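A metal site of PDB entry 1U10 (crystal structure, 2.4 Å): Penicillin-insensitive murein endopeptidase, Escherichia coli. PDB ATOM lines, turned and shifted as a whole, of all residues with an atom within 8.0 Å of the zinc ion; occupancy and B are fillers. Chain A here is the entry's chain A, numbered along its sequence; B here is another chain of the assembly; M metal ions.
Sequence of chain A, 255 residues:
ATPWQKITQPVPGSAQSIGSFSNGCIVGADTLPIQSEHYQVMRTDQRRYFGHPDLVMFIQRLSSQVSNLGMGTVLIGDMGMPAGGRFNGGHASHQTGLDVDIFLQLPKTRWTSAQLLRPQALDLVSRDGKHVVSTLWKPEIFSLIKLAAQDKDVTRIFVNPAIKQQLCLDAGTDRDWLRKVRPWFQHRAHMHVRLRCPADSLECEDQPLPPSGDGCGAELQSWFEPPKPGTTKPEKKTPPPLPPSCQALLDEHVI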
ATOM      1  N   SER A 126     -12.067  14.573 -21.299  1.00  0.00           N
ATOM      2  CA  SER A 126     -10.935  13.843 -20.724  1.00  0.00           C
ATOM      3  C   SER A 126     -10.185  14.624 -19.637  1.00  0.00           C
ATOM      4  O   SER A 126     -10.190  15.854 -19.602  1.00  0.00           O
ATOM      5  CB  SER A 126      -9.937  13.483 -21.808  1.00  0.00           C
ATOM      6  OG  SER A 126      -9.284  14.652 -22.278  1.00  0.00           O
ATOM      7  N   ARG A 127      -9.530  13.867 -18.778  1.00  0.00           N
ATOM      8  CA  ARG A 127      -8.767  14.418 -17.674  1.00  0.00           C
ATOM      9  C   ARG A 127      -7.783  15.479 -18.166  1.00  0.00           C
ATOM     10  O   ARG A 127      -7.618  16.507 -17.518  1.00  0.00           O
ATOM     11  CB  ARG A 127      -8.041  13.275 -16.952  1.00  0.00           C
ATOM     12  CG  ARG A 127      -8.979  12.090 -16.661  1.00  0.00           C
ATOM     13  CD  ARG A 127      -8.383  10.946 -15.842  1.00  0.00           C
ATOM     14  NE  ARG A 127      -7.147  10.398 -16.391  1.00  0.00           N
ATOM     15  CZ  ARG A 127      -6.962  10.020 -17.659  1.00  0.00           C
ATOM     16  NH1 ARG A 127      -7.943  10.127 -18.558  1.00  0.00           N
ATOM     17  NH2 ARG A 127      -5.794   9.517 -18.033  1.00  0.00           N
ATOM     18  N   ASP A 128      -7.131  15.273 -19.294  1.00  0.00           N
ATOM     19  CA  ASP A 128      -6.214  16.336 -19.681  1.00  0.00           C
ATOM     20  C   ASP A 128      -6.949  17.511 -20.329  1.00  0.00           C
ATOM     21  O   ASP A 128      -6.362  18.570 -20.536  1.00  0.00           O
ATOM     22  CB  ASP A 128      -5.117  15.833 -20.579  1.00  0.00           C
ATOM     23  CG  ASP A 128      -5.591  15.529 -21.981  1.00  0.00           C
ATOM     24  OD1 ASP A 128      -6.643  16.046 -22.385  1.00  0.00           O
ATOM     25  OD2 ASP A 128      -4.897  14.768 -22.691  1.00  0.00           O
ATOM     26  N   GLY A 129      -8.229  17.303 -20.659  1.00  0.00           N
ATOM     27  CA  GLY A 129      -9.051  18.353 -21.239  1.00  0.00           C
ATOM     28  C   GLY A 129      -8.986  18.583 -22.741  1.00  0.00           C
ATOM     29  O   GLY A 129      -9.631  19.509 -23.233  1.00  0.00           O
ATOM     30  N   LYS A 130      -8.261  17.742 -23.451  1.00  0.00           N
ATOM     31  CA  LYS A 130      -8.119  17.938 -24.878  1.00  0.00           C
ATOM     32  C   LYS A 130      -8.996  17.061 -25.778  1.00  0.00           C
ATOM     33  O   LYS A 130      -8.928  17.201 -26.997  1.00  0.00           O
ATOM     34  CB  LYS A 130      -6.654  17.753 -25.297  1.00  0.00           C
ATOM     35  CG  LYS A 130      -5.631  18.332 -24.322  1.00  0.00           C
ATOM     36  CD  LYS A 130      -4.596  19.170 -25.064  1.00  0.00           C
ATOM     37  CE  LYS A 130      -3.439  19.589 -24.161  1.00  0.00           C
ATOM     38  NZ  LYS A 130      -2.431  20.431 -24.884  1.00  0.00           N
ATOM     39  N   HIS A 131      -9.819  16.196 -25.206  1.00  0.00           N
ATOM     40  CA  HIS A 131     -10.655  15.317 -26.001  1.00  0.00           C
ATOM     41  C   HIS A 131     -11.713  14.650 -25.161  1.00  0.00           C
ATOM     42  O   HIS A 131     -11.602  14.643 -23.935  1.00  0.00           O
ATOM     43  CB  HIS A 131      -9.784  14.220 -26.641  1.00  0.00           C
ATOM     44  CG  HIS A 131      -8.755  13.696 -25.713  1.00  0.00           C
ATOM     45  ND1 HIS A 131      -8.993  12.659 -24.833  1.00  0.00           N
ATOM     46  CD2 HIS A 131      -7.490  14.096 -25.456  1.00  0.00           C
ATOM     47  CE1 HIS A 131      -7.891  12.395 -24.143  1.00  0.00           C
ATOM     48  NE2 HIS A 131      -6.953  13.272 -24.484  1.00  0.00           N
ATOM     49  N   VAL A 132     -12.722  14.105 -25.810  1.00  0.00           N
ATOM     50  CA  VAL A 132     -13.817  13.467 -25.098  1.00  0.00           C
ATOM     51  C   VAL A 132     -13.505  12.018 -24.749  1.00  0.00           C
ATOM     52  O   VAL A 132     -12.736  11.350 -25.440  1.00  0.00           O
ATOM     53  CB  VAL A 132     -15.095  13.476 -25.930  1.00  0.00           C
ATOM     54  CG1 VAL A 132     -15.364  14.874 -26.440  1.00  0.00           C
ATOM     55  CG2 VAL A 132     -14.979  12.511 -27.091  1.00  0.00           C
ATOM     56  N   SER B 126       1.448  13.696 -29.288  1.00  0.00           N
ATOM     57  CA  SER B 126       1.351  13.863 -27.854  1.00  0.00           C
ATOM     58  C   SER B 126       1.684  12.580 -27.083  1.00  0.00           C
ATOM     59  O   SER B 126       1.646  11.451 -27.580  1.00  0.00           O
ATOM     60  CB  SER B 126      -0.042  14.371 -27.476  1.00  0.00           C
ATOM     61  OG  SER B 126      -0.939  13.294 -27.275  1.00  0.00           O
ATOM     62  N   ARG B 127       2.023  12.818 -25.825  1.00  0.00           N
ATOM     63  CA  ARG B 127       2.413  11.845 -24.835  1.00  0.00           C
ATOM     64  C   ARG B 127       1.389  10.754 -24.650  1.00  0.00           C
ATOM     65  O   ARG B 127       1.726   9.637 -24.262  1.00  0.00           O
ATOM     66  CB  ARG B 127       2.635  12.610 -23.525  1.00  0.00           C
ATOM     67  CG  ARG B 127       3.468  13.883 -23.741  1.00  0.00           C
ATOM     68  CD  ARG B 127       2.885  14.839 -24.802  1.00  0.00           C
ATOM     69  NE  ARG B 127       1.976  15.839 -24.279  1.00  0.00           N
ATOM     70  CZ  ARG B 127       1.888  17.073 -24.746  1.00  0.00           C
ATOM     71  NH1 ARG B 127       2.666  17.473 -25.748  1.00  0.00           N
ATOM     72  NH2 ARG B 127       1.041  17.906 -24.200  1.00  0.00           N
ATOM     73  N   ASP B 128       0.117  11.064 -24.903  1.00  0.00           N
ATOM     74  CA  ASP B 128      -0.908  10.053 -24.750  1.00  0.00           C
ATOM     75  C   ASP B 128      -1.347   9.511 -26.102  1.00  0.00           C
ATOM     76  O   ASP B 128      -2.066   8.515 -26.184  1.00  0.00           O
ATOM     77  CB  ASP B 128      -2.122  10.607 -24.007  1.00  0.00           C
ATOM     78  CG  ASP B 128      -2.933  11.549 -24.860  1.00  0.00           C
ATOM     79  OD1 ASP B 128      -2.668  11.589 -26.084  1.00  0.00           O
ATOM     80  OD2 ASP B 128      -3.825  12.231 -24.303  1.00  0.00           O
ATOM     81  N   GLY B 129      -0.942  10.182 -27.168  1.00  0.00           N
ATOM     82  CA  GLY B 129      -1.282   9.688 -28.477  1.00  0.00           C
ATOM     83  C   GLY B 129      -2.576  10.194 -29.065  1.00  0.00           C
ATOM     84  O   GLY B 129      -3.019   9.641 -30.076  1.00  0.00           O
ATOM     85  N   LYS B 130      -3.205  11.232 -28.500  1.00  0.00           N
ATOM     86  CA  LYS B 130      -4.455  11.651 -29.145  1.00  0.00           C
ATOM     87  C   LYS B 130      -4.366  13.035 -29.796  1.00  0.00           C
ATOM     88  O   LYS B 130      -5.326  13.498 -30.417  1.00  0.00           O
ATOM     89  CB  LYS B 130      -5.572  11.715 -28.105  1.00  0.00           C
ATOM     90  CG  LYS B 130      -5.511  10.627 -27.067  1.00  0.00           C
ATOM     91  CD  LYS B 130      -6.748   9.791 -27.140  1.00  0.00           C
ATOM     92  CE  LYS B 130      -7.200   9.378 -25.748  1.00  0.00           C
ATOM     93  NZ  LYS B 130      -8.547   8.703 -25.788  1.00  0.00           N
ATOM     94  N   HIS B 131      -3.235  13.710 -29.601  1.00  0.00           N
ATOM     95  CA  HIS B 131      -3.065  15.035 -30.160  1.00  0.00           C
ATOM     96  C   HIS B 131      -1.605  15.306 -30.544  1.00  0.00           C
ATOM     97  O   HIS B 131      -0.714  14.506 -30.249  1.00  0.00           O
ATOM     98  CB  HIS B 131      -3.646  16.095 -29.257  1.00  0.00           C
ATOM     99  CG  HIS B 131      -3.597  15.756 -27.743  1.00  0.00           C
ATOM    100  ND1 HIS B 131      -2.569  16.151 -26.942  1.00  0.00           N
ATOM    101  CD2 HIS B 131      -4.455  15.091 -26.985  1.00  0.00           C
ATOM    102  CE1 HIS B 131      -2.805  15.705 -25.736  1.00  0.00           C
ATOM    103  NE2 HIS B 131      -3.928  15.077 -25.744  1.00  0.00           N
HETATM  104 ZN    ZN M   1      -5.101  14.084 -24.409  1.00  0.00          ZN
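The zinc ion is bound by the side-chain carboxylate (OD2) of Asp 128 of chain A (1.9 Å).
NE2 of His 131 of chain A is bound to the zinc ion (2.0 Å).
NE2 of His 131 of chain B is bound to the zinc ion.
The zinc ion is bound by OD2 of Asp 128 of chain B.
The zinc ion has four donor atoms within binding distance.
OD1 of Asp 128 of chain A lies within hydrogen-bond range of N of Lys 130 of chain A, at 2.6 Å.
OD1 of Asp 128 of chain A lies within hydrogen-bond range of OG of Ser 126 of chain A.
N of Ser 126 of chain A lies within hydrogen-bond range of O of His 131 of chain A (2.7 Å).
The backbone carbonyl oxygen of His 131 of chain B is in hydrogen-bond range of the backbone NH of Ser 126 of chain B, 2.5 Å away.
OD1 of Asp 128 of chain B is in hydrogen-bond range of N of Lys 130 of chain B (2.5 Å).
The side-chain hydroxyl (OG) of Ser 126 of chain B sits at hydrogen-bond distance from the side-chain carboxylate (OD1) of Asp 128 of chain B (2.7 Å).
The nearest printed residue that does not touch the zinc ion is Lys 130 of chain A (4.1 Å).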
